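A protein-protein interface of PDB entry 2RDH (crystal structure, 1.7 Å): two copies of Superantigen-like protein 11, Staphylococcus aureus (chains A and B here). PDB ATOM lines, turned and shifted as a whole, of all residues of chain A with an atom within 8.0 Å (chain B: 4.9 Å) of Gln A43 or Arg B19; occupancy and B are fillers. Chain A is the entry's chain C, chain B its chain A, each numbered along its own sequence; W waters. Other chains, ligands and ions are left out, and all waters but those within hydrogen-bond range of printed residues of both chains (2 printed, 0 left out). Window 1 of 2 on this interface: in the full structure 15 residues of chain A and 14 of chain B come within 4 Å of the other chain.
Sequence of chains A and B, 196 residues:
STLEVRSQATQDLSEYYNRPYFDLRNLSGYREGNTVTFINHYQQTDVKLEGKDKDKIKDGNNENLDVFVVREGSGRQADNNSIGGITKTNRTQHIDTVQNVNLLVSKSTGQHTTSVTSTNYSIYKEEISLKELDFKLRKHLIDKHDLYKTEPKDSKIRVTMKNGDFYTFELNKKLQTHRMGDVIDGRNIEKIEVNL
Water W2 bridges the backbone carbonyl oxygen (O) of Asn B18 (2.9 Å) and the side-chain amide nitrogen (ND2) of Asn A80 (3.0 Å).
Water W1 lies within hydrogen-bond range of O of Glu B15 (2.9 Å), O of Asn B18 (3.0 Å) and ND2 of Asn A40 (3.5 Å).
Of the 22 printed residues of chain A, 8 touch a printed residue of chain B.
Printed residues of chain A that touch a printed residue of chain B: Phe A22, Leu A24, Asn A40, Tyr A42, Gln A43, Arg A71, Ala A78 and Asn A80.
Hydrophobic or aromatic side chains of chain A within 4 Å of the printed part of chain B: Phe A22, Leu A24, Tyr A42 and Ala A78.
Printed residues of chain B that touch a printed residue of chain A: Glu B15, Tyr B16, Asn B18, Arg B19, Pro B20 and Arg B71.
Along chain B the printed residues that touch a printed residue of chain A span positions 15 to 71.
Among the printed residues, no Asp or Glu carboxylate lies within 4 Å of a Lys or Arg side-chain nitrogen of the other chain.
Among the printed residues, pairs that only touch across the chains: Phe A22 with Asn B18, Phe A22 with Arg B19, Phe A22 with Pro B20, Leu A24 with Asn B18, Asn A40 with Glu B15, Tyr A42 with Glu B15, Tyr A42 with Tyr B16, Gln A43 with Arg B19, Gln A43 with Pro B20, Arg A71 with Pro B20, Ala A78 with Arg B71 and Asn A80 with Pro B20.
Of the printed residues of chain B, Tyr A42 touches Glu B15 (3.5 Å), Tyr B16 (3.5 Å) and Arg B19 (3.3 Å).
Gln A43 touches two residues of chain B.
Val A69 touches none of the printed residues of chain B.
Of the printed residues of chain B, Arg A71 touches Pro B20.
Of the printed residues of chain B, Ala A78 touches Arg B71 (3.5 Å).
Printed residues of chain B within 4 Å of Asn A80: Pro B20 (3.7 Å).
Of the printed residues of chain A, Asn B18 touches Phe A22 (3.6 Å) and Leu A24 (3.9 Å).
Arg B19 touches just these residues of chain A: Phe A22, Tyr A42 and Gln A43.
The nearest residue of chain A that does not touch Arg B19 is Asn A40 (5.3 Å).
The nearest printed residue of chain B that does not touch Ala A78 is Pro B20 (4.9 Å).
The side-chain amide oxygen of Asn A40 lies within hydrogen-bond range of the backbone NH of Gln A43 (2.7 Å).
The backbone NH (N) of Asn A80 sits close to the side-chain amide nitrogen (NE2) of Gln A43, 3.3 Å away.
The side-chain amide nitrogen (ND2) of Asn A80 is in hydrogen-bond range of the side-chain hydroxyl (OG1) of Thr A45, 3.2 Å away.
The backbone carbonyl oxygen (O) of Asn A80 is in hydrogen-bond range of the backbone NH (N) of Asp A46 (2.7 Å).
O of Gln A77 sits at hydrogen-bond distance from NH2 of Arg A71 (2.7 Å).
The guanidinium group of Arg A71 is in hydrogen-bond range of the side-chain amide oxygen of Asn A80 (2.7 Å).
Arg A71 touches Pro B20, but with the chains exchanged Pro A20 does not touch Arg B71 (13.4 Å).
3 positions are printed for both chains.
Of the 13 pairs that touch across the chains among the printed residues, none has its exchanged pair printed and touching as well.
The backbone carbonyl oxygen (O) of Tyr A42 lies within hydrogen-bond range of the guanidinium group (NH1) of Arg B19 (3.3 Å).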
ATOM      1  N   PRO A  20     -10.190  16.254  10.636  1.00  0.00           N
ATOM      2  CA  PRO A  20     -11.157  15.294  11.190  1.00  0.00           C
ATOM      3  C   PRO A  20     -11.099  15.287  12.719  1.00  0.00           C
ATOM      4  O   PRO A  20     -10.055  15.657  13.304  1.00  0.00           O
ATOM      5  CB  PRO A  20     -10.636  13.931  10.677  1.00  0.00           C
ATOM      6  CG  PRO A  20      -9.169  14.119  10.505  1.00  0.00           C
ATOM      7  CD  PRO A  20      -9.026  15.578  10.033  1.00  0.00           C
ATOM      8  N   TYR A  21     -12.199  14.898  13.374  1.00  0.00           N
ATOM      9  CA  TYR A  21     -12.154  14.638  14.810  1.00  0.00           C
ATOM     10  C   TYR A  21     -12.518  13.184  15.014  1.00  0.00           C
ATOM     11  O   TYR A  21     -13.037  12.540  14.099  1.00  0.00           O
ATOM     12  CB  TYR A  21     -13.146  15.539  15.575  1.00  0.00           C
ATOM     13  CG  TYR A  21     -14.589  15.260  15.151  1.00  0.00           C
ATOM     14  CD1 TYR A  21     -15.335  14.253  15.788  1.00  0.00           C
ATOM     15  CD2 TYR A  21     -15.202  15.994  14.119  1.00  0.00           C
ATOM     16  CE1 TYR A  21     -16.637  13.969  15.406  1.00  0.00           C
ATOM     17  CE2 TYR A  21     -16.540  15.722  13.737  1.00  0.00           C
ATOM     18  CZ  TYR A  21     -17.243  14.706  14.408  1.00  0.00           C
ATOM     19  OH  TYR A  21     -18.550  14.361  14.057  1.00  0.00           O
ATOM     20  N   PHE A  22     -12.244  12.685  16.212  1.00  0.00           N
ATOM     21  CA  PHE A  22     -12.503  11.278  16.528  1.00  0.00           C
ATOM     22  C   PHE A  22     -13.149  11.298  17.893  1.00  0.00           C
ATOM     23  O   PHE A  22     -12.504  11.587  18.910  1.00  0.00           O
ATOM     24  CB  PHE A  22     -11.208  10.426  16.476  1.00  0.00           C
ATOM     25  CG  PHE A  22     -10.410  10.641  15.197  1.00  0.00           C
ATOM     26  CD1 PHE A  22      -9.442  11.667  15.123  1.00  0.00           C
ATOM     27  CD2 PHE A  22     -10.670   9.873  14.051  1.00  0.00           C
ATOM     28  CE1 PHE A  22      -8.726  11.881  13.925  1.00  0.00           C
ATOM     29  CE2 PHE A  22      -9.949  10.062  12.868  1.00  0.00           C
ATOM     30  CZ  PHE A  22      -9.007  11.096  12.783  1.00  0.00           C
ATOM     31  N   LEU A  24     -14.322   9.381  20.629  1.00  0.00           N
ATOM     32  CA  LEU A  24     -14.130   8.018  21.174  1.00  0.00           C
ATOM     33  C   LEU A  24     -14.947   7.863  22.442  1.00  0.00           C
ATOM     34  O   LEU A  24     -14.878   8.727  23.346  1.00  0.00           O
ATOM     35  CB  LEU A  24     -12.644   7.783  21.506  1.00  0.00           C
ATOM     36  CG  LEU A  24     -11.605   8.108  20.429  1.00  0.00           C
ATOM     37  CD1 LEU A  24     -10.208   7.756  20.930  1.00  0.00           C
ATOM     38  CD2 LEU A  24     -11.897   7.366  19.116  1.00  0.00           C
ATOM     39  N   LEU A  27     -14.153   4.530  27.124  1.00  0.00           N
ATOM     40  CA  LEU A  27     -12.869   3.836  27.161  1.00  0.00           C
ATOM     41  C   LEU A  27     -12.013   4.242  28.379  1.00  0.00           C
ATOM     42  O   LEU A  27     -12.318   5.241  29.050  1.00  0.00           O
ATOM     43  CB  LEU A  27     -12.139   4.037  25.823  1.00  0.00           C
ATOM     44  CG  LEU A  27     -11.796   5.429  25.283  1.00  0.00           C
ATOM     45  CD1 LEU A  27     -10.911   5.320  24.059  1.00  0.00           C
ATOM     46  CD2 LEU A  27     -13.021   6.256  24.939  1.00  0.00           C
ATOM     47  N   THR A  37      -3.201   8.539  28.258  1.00  0.00           N
ATOM     48  CA  THR A  37      -3.000   7.664  27.120  1.00  0.00           C
ATOM     49  C   THR A  37      -4.169   6.702  26.988  1.00  0.00           C
ATOM     50  O   THR A  37      -4.585   6.081  27.970  1.00  0.00           O
ATOM     51  CB  THR A  37      -1.668   6.887  27.252  1.00  0.00           C
ATOM     52  OG1 THR A  37      -0.589   7.823  27.402  1.00  0.00           O
ATOM     53  CG2 THR A  37      -1.428   6.033  26.021  1.00  0.00           C
ATOM     54  N   PHE A  38      -4.698   6.608  25.770  1.00  0.00           N
ATOM     55  CA  PHE A  38      -5.756   5.674  25.436  1.00  0.00           C
ATOM     56  C   PHE A  38      -5.197   4.755  24.364  1.00  0.00           C
ATOM     57  O   PHE A  38      -4.590   5.225  23.402  1.00  0.00           O
ATOM     58  CB  PHE A  38      -6.965   6.418  24.872  1.00  0.00           C
ATOM     59  CG  PHE A  38      -7.581   7.397  25.823  1.00  0.00           C
ATOM     60  CD1 PHE A  38      -7.049   8.691  25.965  1.00  0.00           C
ATOM     61  CD2 PHE A  38      -8.699   7.038  26.576  1.00  0.00           C
ATOM     62  CE1 PHE A  38      -7.609   9.602  26.848  1.00  0.00           C
ATOM     63  CE2 PHE A  38      -9.281   7.954  27.467  1.00  0.00           C
ATOM     64  CZ  PHE A  38      -8.727   9.230  27.614  1.00  0.00           C
ATOM     65  N   ILE A  39      -5.396   3.452  24.524  1.00  0.00           N
ATOM     66  CA  ILE A  39      -4.759   2.481  23.644  1.00  0.00           C
ATOM     67  C   ILE A  39      -5.758   1.434  23.168  1.00  0.00           C
ATOM     68  O   ILE A  39      -6.481   0.847  23.974  1.00  0.00           O
ATOM     69  CB  ILE A  39      -3.525   1.800  24.336  1.00  0.00           C
ATOM     70  CG1 ILE A  39      -2.515   2.868  24.793  1.00  0.00           C
ATOM     71  CG2 ILE A  39      -2.876   0.740  23.414  1.00  0.00           C
ATOM     72  CD1 ILE A  39      -1.274   2.329  25.482  1.00  0.00           C
ATOM     73  N   ASN A  40      -5.801   1.223  21.859  1.00  0.00           N
ATOM     74  CA  ASN A  40      -6.434   0.021  21.309  1.00  0.00           C
ATOM     75  C   ASN A  40      -5.488  -0.675  20.333  1.00  0.00           C
ATOM     76  O   ASN A  40      -4.396  -0.158  20.022  1.00  0.00           O
ATOM     77  CB  ASN A  40      -7.823   0.323  20.715  1.00  0.00           C
ATOM     78  CG  ASN A  40      -7.767   1.234  19.516  1.00  0.00           C
ATOM     79  OD1 ASN A  40      -7.040   0.968  18.559  1.00  0.00           O
ATOM     80  ND2 ASN A  40      -8.539   2.328  19.552  1.00  0.00           N
ATOM     81  N   HIS A  41      -5.870  -1.857  19.861  1.00  0.00           N
ATOM     82  CA  HIS A  41      -5.005  -2.579  18.931  1.00  0.00           C
ATOM     83  C   HIS A  41      -4.628  -1.738  17.707  1.00  0.00           C
ATOM     84  O   HIS A  41      -3.518  -1.864  17.183  1.00  0.00           O
ATOM     85  CB  HIS A  41      -5.664  -3.876  18.471  1.00  0.00           C
ATOM     86  CG  HIS A  41      -4.922  -4.568  17.371  1.00  0.00           C
ATOM     87  ND1 HIS A  41      -3.689  -5.158  17.562  1.00  0.00           N
ATOM     88  CD2 HIS A  41      -5.226  -4.747  16.064  1.00  0.00           C
ATOM     89  CE1 HIS A  41      -3.274  -5.686  16.425  1.00  0.00           C
ATOM     90  NE2 HIS A  41      -4.187  -5.452  15.499  1.00  0.00           N
ATOM     91  N   TYR A  42      -5.546  -0.877  17.262  1.00  0.00           N
ATOM     92  CA  TYR A  42      -5.357  -0.157  16.008  1.00  0.00           C
ATOM     93  C   TYR A  42      -4.717   1.214  16.177  1.00  0.00           C
ATOM     94  O   TYR A  42      -4.154   1.737  15.229  1.00  0.00           O
ATOM     95  CB  TYR A  42      -6.690   0.017  15.268  1.00  0.00           C
ATOM     96  CG  TYR A  42      -7.392  -1.247  14.834  1.00  0.00           C
ATOM     97  CD1 TYR A  42      -8.573  -1.650  15.447  1.00  0.00           C
ATOM     98  CD2 TYR A  42      -6.880  -2.034  13.801  1.00  0.00           C
ATOM     99  CE1 TYR A  42      -9.233  -2.813  15.048  1.00  0.00           C
ATOM    100  CE2 TYR A  42      -7.524  -3.192  13.395  1.00  0.00           C
ATOM    101  CZ  TYR A  42      -8.700  -3.573  14.016  1.00  0.00           C
ATOM    102  OH  TYR A  42      -9.338  -4.732  13.613  1.00  0.00           O
ATOM    103  N   GLN A  43      -4.810   1.804  17.370  1.00  0.00           N
ATOM    104  CA  GLN A  43      -4.555   3.247  17.532  1.00  0.00           C
ATOM    105  C   GLN A  43      -4.212   3.630  18.970  1.00  0.00           C
ATOM    106  O   GLN A  43      -4.932   3.230  19.885  1.00  0.00           O
ATOM    107  CB  GLN A  43      -5.797   4.033  17.082  1.00  0.00           C
ATOM    108  CG  GLN A  43      -5.686   5.554  17.195  1.00  0.00           C
ATOM    109  CD  GLN A  43      -4.738   6.139  16.167  1.00  0.00           C
ATOM    110  OE1 GLN A  43      -4.934   5.986  14.969  1.00  0.00           O
ATOM    111  NE2 GLN A  43      -3.672   6.774  16.640  1.00  0.00           N
ATOM    112  N   GLN A  44      -3.116   4.372  19.166  1.00  0.00           N
ATOM    113  CA  GLN A  44      -2.839   5.015  20.465  1.00  0.00           C
ATOM    114  C   GLN A  44      -3.159   6.518  20.411  1.00  0.00           C
ATOM    115  O   GLN A  44      -2.861   7.184  19.424  1.00  0.00           O
ATOM    116  CB  GLN A  44      -1.395   4.812  20.919  1.00  0.00           C
ATOM    117  CG  GLN A  44      -1.016   5.586  22.193  1.00  0.00           C
ATOM    118  CD  GLN A  44       0.359   5.223  22.763  1.00  0.00           C
ATOM    119  OE1 GLN A  44       0.846   4.094  22.612  1.00  0.00           O
ATOM    120  NE2 GLN A  44       0.980   6.178  23.434  1.00  0.00           N
ATOM    121  N   THR A  45      -3.765   7.027  21.482  1.00  0.00           N
ATOM    122  CA  THR A  45      -4.116   8.434  21.587  1.00  0.00           C
ATOM    123  C   THR A  45      -3.527   9.008  22.883  1.00  0.00           C
ATOM    124  O   THR A  45      -3.768   8.466  23.961  1.00  0.00           O
ATOM    125  CB  THR A  45      -5.662   8.598  21.560  1.00  0.00           C
ATOM    126  OG1 THR A  45      -6.177   8.065  20.327  1.00  0.00           O
ATOM    127  CG2 THR A  45      -6.062  10.065  21.710  1.00  0.00           C
ATOM    128  N   ASP A  46      -2.757  10.089  22.766  1.00  0.00           N
ATOM    129  CA  ASP A  46      -2.056  10.714  23.890  1.00  0.00           C
ATOM    130  C   ASP A  46      -2.680  12.082  24.064  1.00  0.00           C
ATOM    131  O   ASP A  46      -2.616  12.920  23.156  1.00  0.00           O
ATOM    132  CB  ASP A  46      -0.563  10.908  23.597  1.00  0.00           C
ATOM    133  CG  ASP A  46       0.121   9.636  23.131  1.00  0.00           C
ATOM    134  OD1 ASP A  46      -0.105   8.581  23.736  1.00  0.00           O
ATOM    135  OD2 ASP A  46       0.878   9.704  22.146  1.00  0.00           O
ATOM    136  N   VAL A  69     -11.163  13.794  20.112  1.00  0.00           N
ATOM    137  CA  VAL A  69      -9.769  13.880  19.661  1.00  0.00           C
ATOM    138  C   VAL A  69      -9.629  14.736  18.421  1.00  0.00           C
ATOM    139  O   VAL A  69     -10.371  14.574  17.466  1.00  0.00           O
ATOM    140  CB  VAL A  69      -9.216  12.468  19.342  1.00  0.00           C
ATOM    141  CG1 VAL A  69      -7.774  12.531  18.743  1.00  0.00           C
ATOM    142  CG2 VAL A  69      -9.293  11.520  20.584  1.00  0.00           C
ATOM    143  N   ARG A  71      -6.198  15.889  16.017  1.00  0.00           N
ATOM    144  CA  ARG A  71      -4.744  15.671  15.962  1.00  0.00           C
ATOM    145  C   ARG A  71      -4.004  16.997  15.858  1.00  0.00           C
ATOM    146  O   ARG A  71      -4.305  17.802  14.980  1.00  0.00           O
ATOM    147  CB  ARG A  71      -4.379  14.784  14.788  1.00  0.00           C
ATOM    148  CG  ARG A  71      -4.756  13.331  15.015  1.00  0.00           C
ATOM    149  CD  ARG A  71      -4.829  12.520  13.695  1.00  0.00           C
ATOM    150  NE  ARG A  71      -3.524  12.493  13.054  1.00  0.00           N
ATOM    151  CZ  ARG A  71      -2.546  11.630  13.344  1.00  0.00           C
ATOM    152  NH1 ARG A  71      -2.694  10.671  14.265  1.00  0.00           N
ATOM    153  NH2 ARG A  71      -1.402  11.741  12.699  1.00  0.00           N
ATOM    154  N   GLN A  77       2.238  11.474  12.358  1.00  0.00           N
ATOM    155  CA  GLN A  77       2.462  10.571  13.514  1.00  0.00           C
ATOM    156  C   GLN A  77       1.429   9.457  13.558  1.00  0.00           C
ATOM    157  O   GLN A  77       0.246   9.701  13.350  1.00  0.00           O
ATOM    158  CB  GLN A  77       2.427  11.318  14.870  1.00  0.00           C
ATOM    159  CG  GLN A  77       3.163  12.646  14.931  1.00  0.00           C
ATOM    160  CD  GLN A  77       2.254  13.790  14.585  1.00  0.00           C
ATOM    161  OE1 GLN A  77       1.572  13.761  13.559  1.00  0.00           O
ATOM    162  NE2 GLN A  77       2.204  14.803  15.451  1.00  0.00           N
ATOM    163  N   ALA A  78       1.891   8.248  13.869  1.00  0.00           N
ATOM    164  CA  ALA A  78       1.019   7.108  14.086  1.00  0.00           C
ATOM    165  C   ALA A  78       0.024   7.399  15.211  1.00  0.00           C
ATOM    166  O   ALA A  78      -1.182   7.272  15.010  1.00  0.00           O
ATOM    167  CB  ALA A  78       1.833   5.868  14.388  1.00  0.00           C
ATOM    168  N   ASP A  79       0.525   7.833  16.371  1.00  0.00           N
ATOM    169  CA  ASP A  79      -0.328   8.143  17.508  1.00  0.00           C
ATOM    170  C   ASP A  79      -1.129   9.442  17.322  1.00  0.00           C
ATOM    171  O   ASP A  79      -0.711  10.350  16.608  1.00  0.00           O
ATOM    172  CB  ASP A  79       0.488   8.221  18.799  1.00  0.00           C
ATOM    173  CG  ASP A  79       1.189   6.907  19.145  1.00  0.00           C
ATOM    174  OD1 ASP A  79       0.814   5.834  18.614  1.00  0.00           O
ATOM    175  OD2 ASP A  79       2.127   6.963  19.964  1.00  0.00           O
ATOM    176  N   ASN A  80      -2.291   9.510  17.952  1.00  0.00           N
ATOM    177  CA  ASN A  80      -3.010  10.797  18.014  1.00  0.00           C
ATOM    178  C   ASN A  80      -2.482  11.624  19.172  1.00  0.00           C
ATOM    179  O   ASN A  80      -2.523  11.170  20.312  1.00  0.00           O
ATOM    180  CB  ASN A  80      -4.502  10.596  18.229  1.00  0.00           C
ATOM    181  CG  ASN A  80      -5.179   9.906  17.055  1.00  0.00           C
ATOM    182  OD1 ASN A  80      -4.790  10.084  15.901  1.00  0.00           O
ATOM    183  ND2 ASN A  80      -6.221   9.123  17.352  1.00  0.00           N
ATOM    184  N   ASN A  81      -1.980  12.822  18.880  1.00  0.00           N
ATOM    185  CA  ASN A  81      -1.625  13.785  19.923  1.00  0.00           C
ATOM    186  C   ASN A  81      -2.680  14.887  19.964  1.00  0.00           C
ATOM    187  O   ASN A  81      -2.853  15.632  19.020  1.00  0.00           O
ATOM    188  CB  ASN A  81      -0.230  14.370  19.702  1.00  0.00           C
ATOM    189  CG  ASN A  81       0.859  13.294  19.721  1.00  0.00           C
ATOM    190  OD1 ASN A  81       1.098  12.645  20.752  1.00  0.00           O
ATOM    191  ND2 ASN A  81       1.510  13.085  18.571  1.00  0.00           N
ATOM    192  N   GLU B  15     -13.140   0.713  16.115  1.00  0.00           N
ATOM    193  CA  GLU B  15     -11.718   0.969  16.302  1.00  0.00           C
ATOM    194  C   GLU B  15     -10.969   1.044  14.996  1.00  0.00           C
ATOM    195  O   GLU B  15     -10.123   1.931  14.827  1.00  0.00           O
ATOM    196  CB  GLU B  15     -11.084  -0.060  17.217  1.00  0.00           C
ATOM    197  CG  GLU B  15     -11.553   0.144  18.661  1.00  0.00           C
ATOM    198  CD  GLU B  15     -11.089  -0.939  19.609  1.00  0.00           C
ATOM    199  OE1 GLU B  15     -10.232  -1.768  19.245  1.00  0.00           O
ATOM    200  OE2 GLU B  15     -11.595  -0.926  20.734  1.00  0.00           O
ATOM    201  N   TYR B  16     -11.260   0.120  14.078  1.00  0.00           N
ATOM    202  CA  TYR B  16     -10.555   0.109  12.803  1.00  0.00           C
ATOM    203  C   TYR B  16     -10.865   1.356  11.966  1.00  0.00           C
ATOM    204  O   TYR B  16      -9.943   2.009  11.428  1.00  0.00           O
ATOM    205  CB  TYR B  16     -10.927  -1.154  12.023  1.00  0.00           C
ATOM    206  CG  TYR B  16     -10.232  -1.260  10.680  1.00  0.00           C
ATOM    207  CD1 TYR B  16      -8.955  -1.810  10.574  1.00  0.00           C
ATOM    208  CD2 TYR B  16     -10.852  -0.792   9.512  1.00  0.00           C
ATOM    209  CE1 TYR B  16      -8.319  -1.901   9.343  1.00  0.00           C
ATOM    210  CE2 TYR B  16     -10.226  -0.875   8.261  1.00  0.00           C
ATOM    211  CZ  TYR B  16      -8.954  -1.431   8.187  1.00  0.00           C
ATOM    212  OH  TYR B  16      -8.317  -1.547   6.991  1.00  0.00           O
ATOM    213  N   TYR B  17     -12.142   1.733  11.908  1.00  0.00           N
ATOM    214  CA  TYR B  17     -12.581   2.756  10.975  1.00  0.00           C
ATOM    215  C   TYR B  17     -12.513   4.169  11.565  1.00  0.00           C
ATOM    216  O   TYR B  17     -12.347   5.125  10.821  1.00  0.00           O
ATOM    217  CB  TYR B  17     -14.001   2.465  10.479  1.00  0.00           C
ATOM    218  CG  TYR B  17     -14.008   1.451   9.365  1.00  0.00           C
ATOM    219  CD1 TYR B  17     -14.454   0.145   9.569  1.00  0.00           C
ATOM    220  CD2 TYR B  17     -13.560   1.829   8.096  1.00  0.00           C
ATOM    221  CE1 TYR B  17     -14.453  -0.788   8.498  1.00  0.00           C
ATOM    222  CE2 TYR B  17     -13.539   0.923   7.052  1.00  0.00           C
ATOM    223  CZ  TYR B  17     -14.008  -0.368   7.253  1.00  0.00           C
ATOM    224  OH  TYR B  17     -13.975  -1.218   6.204  1.00  0.00           O
ATOM    225  N   ASN B  18     -12.596   4.299  12.879  1.00  0.00           N
ATOM    226  CA  ASN B  18     -12.606   5.658  13.491  1.00  0.00           C
ATOM    227  C   ASN B  18     -11.179   6.133  13.861  1.00  0.00           C
ATOM    228  O   ASN B  18     -10.851   6.321  15.046  1.00  0.00           O
ATOM    229  CB  ASN B  18     -13.587   5.729  14.684  1.00  0.00           C
ATOM    230  CG  ASN B  18     -13.971   7.198  15.063  1.00  0.00           C
ATOM    231  OD1 ASN B  18     -13.793   8.132  14.266  1.00  0.00           O
ATOM    232  ND2 ASN B  18     -14.525   7.377  16.256  1.00  0.00           N
ATOM    233  N   ARG B  19     -10.378   6.333  12.822  1.00  0.00           N
ATOM    234  CA  ARG B  19      -8.943   6.561  12.919  1.00  0.00           C
ATOM    235  C   ARG B  19      -8.473   7.417  11.762  1.00  0.00           C
ATOM    236  O   ARG B  19      -9.113   7.433  10.715  1.00  0.00           O
ATOM    237  CB  ARG B  19      -8.188   5.243  12.769  1.00  0.00           C
ATOM    238  CG  ARG B  19      -8.241   4.328  13.953  1.00  0.00           C
ATOM    239  CD  ARG B  19      -7.230   3.175  13.707  1.00  0.00           C
ATOM    240  NE  ARG B  19      -7.528   2.305  12.571  1.00  0.00           N
ATOM    241  CZ  ARG B  19      -6.596   1.673  11.850  1.00  0.00           C
ATOM    242  NH1 ARG B  19      -5.308   1.844  12.124  1.00  0.00           N
ATOM    243  NH2 ARG B  19      -6.927   0.861  10.871  1.00  0.00           N
ATOM    244  N   PRO B  20      -7.306   8.069  11.918  1.00  0.00           N
ATOM    245  CA  PRO B  20      -6.748   8.765  10.776  1.00  0.00           C
ATOM    246  C   PRO B  20      -6.263   7.833   9.680  1.00  0.00           C
ATOM    247  O   PRO B  20      -5.902   6.662   9.921  1.00  0.00           O
ATOM    248  CB  PRO B  20      -5.563   9.549  11.384  1.00  0.00           C
ATOM    249  CG  PRO B  20      -5.148   8.740  12.515  1.00  0.00           C
ATOM    250  CD  PRO B  20      -6.445   8.190  13.105  1.00  0.00           C
ATOM    251  N   TYR B  21      -6.280   8.366   8.467  1.00  0.00           N
ATOM    252  CA  TYR B  21      -5.585   7.753   7.323  1.00  0.00           C
ATOM    253  C   TYR B  21      -4.492   8.722   6.895  1.00  0.00           C
ATOM    254  O   TYR B  21      -4.443   9.865   7.389  1.00  0.00           O
ATOM    255  CB  TYR B  21      -6.580   7.514   6.178  1.00  0.00           C
ATOM    256  CG  TYR B  21      -7.218   8.809   5.659  1.00  0.00           C
ATOM    257  CD1 TYR B  21      -6.542   9.625   4.748  1.00  0.00           C
ATOM    258  CD2 TYR B  21      -8.474   9.206   6.084  1.00  0.00           C
ATOM    259  CE1 TYR B  21      -7.075  10.797   4.282  1.00  0.00           C
ATOM    260  CE2 TYR B  21      -9.026  10.400   5.617  1.00  0.00           C
ATOM    261  CZ  TYR B  21      -8.319  11.199   4.738  1.00  0.00           C
ATOM    262  OH  TYR B  21      -8.902  12.372   4.275  1.00  0.00           O
ATOM    263  N   VAL B  70      -3.863   3.187   5.484  1.00  0.00           N
ATOM    264  CA  VAL B  70      -4.468   2.885   6.763  1.00  0.00           C
ATOM    265  C   VAL B  70      -3.563   1.857   7.450  1.00  0.00           C
ATOM    266  O   VAL B  70      -3.357   0.790   6.911  1.00  0.00           O
ATOM    267  CB  VAL B  70      -5.904   2.295   6.586  1.00  0.00           C
ATOM    268  CG1 VAL B  70      -6.462   1.862   7.930  1.00  0.00           C
ATOM    269  CG2 VAL B  70      -6.830   3.342   5.947  1.00  0.00           C
ATOM    270  N   ARG B  71      -3.012   2.216   8.604  1.00  0.00           N
ATOM    271  CA  ARG B  71      -2.104   1.334   9.348  1.00  0.00           C
ATOM    272  C   ARG B  71      -2.867   0.084   9.766  1.00  0.00           C
ATOM    273  O   ARG B  71      -3.909   0.190  10.389  1.00  0.00           O
ATOM    274  CB  ARG B  71      -1.575   2.060  10.582  1.00  0.00           C
ATOM    275  CG  ARG B  71      -0.742   3.307  10.295  1.00  0.00           C
ATOM    276  CD  ARG B  71      -0.335   4.039  11.604  1.00  0.00           C
ATOM    277  NE  ARG B  71       0.337   3.169  12.591  1.00  0.00           N
ATOM    278  CZ  ARG B  71       1.639   2.858  12.581  1.00  0.00           C
ATOM    279  NH1 ARG B  71       2.450   3.311  11.632  1.00  0.00           N
ATOM    280  NH2 ARG B  71       2.148   2.093  13.537  1.00  0.00           N
ATOM    281  N   PHE B 135     -13.367   3.648   3.329  1.00  0.00           N
ATOM    282  CA  PHE B 135     -12.905   4.235   4.569  1.00  0.00           C
ATOM    283  C   PHE B 135     -13.539   5.610   4.845  1.00  0.00           C
ATOM    284  O   PHE B 135     -14.027   5.874   5.957  1.00  0.00           O
ATOM    285  CB  PHE B 135     -11.367   4.264   4.616  1.00  0.00           C
ATOM    286  CG  PHE B 135     -10.779   4.404   6.012  1.00  0.00           C
ATOM    287  CD1 PHE B 135     -10.533   3.257   6.780  1.00  0.00           C
ATOM    288  CD2 PHE B 135     -10.531   5.647   6.572  1.00  0.00           C
ATOM    289  CE1 PHE B 135      -9.986   3.345   8.050  1.00  0.00           C
ATOM    290  CE2 PHE B 135      -9.997   5.737   7.885  1.00  0.00           C
ATOM    291  CZ  PHE B 135      -9.726   4.596   8.595  1.00  0.00           C
HETATM  292  O   HOH W   1      -9.971   4.027  16.850  1.00  0.00           O
HETATM  293  O   HOH W   2      -8.661   7.808  16.243  1.00  0.00           O
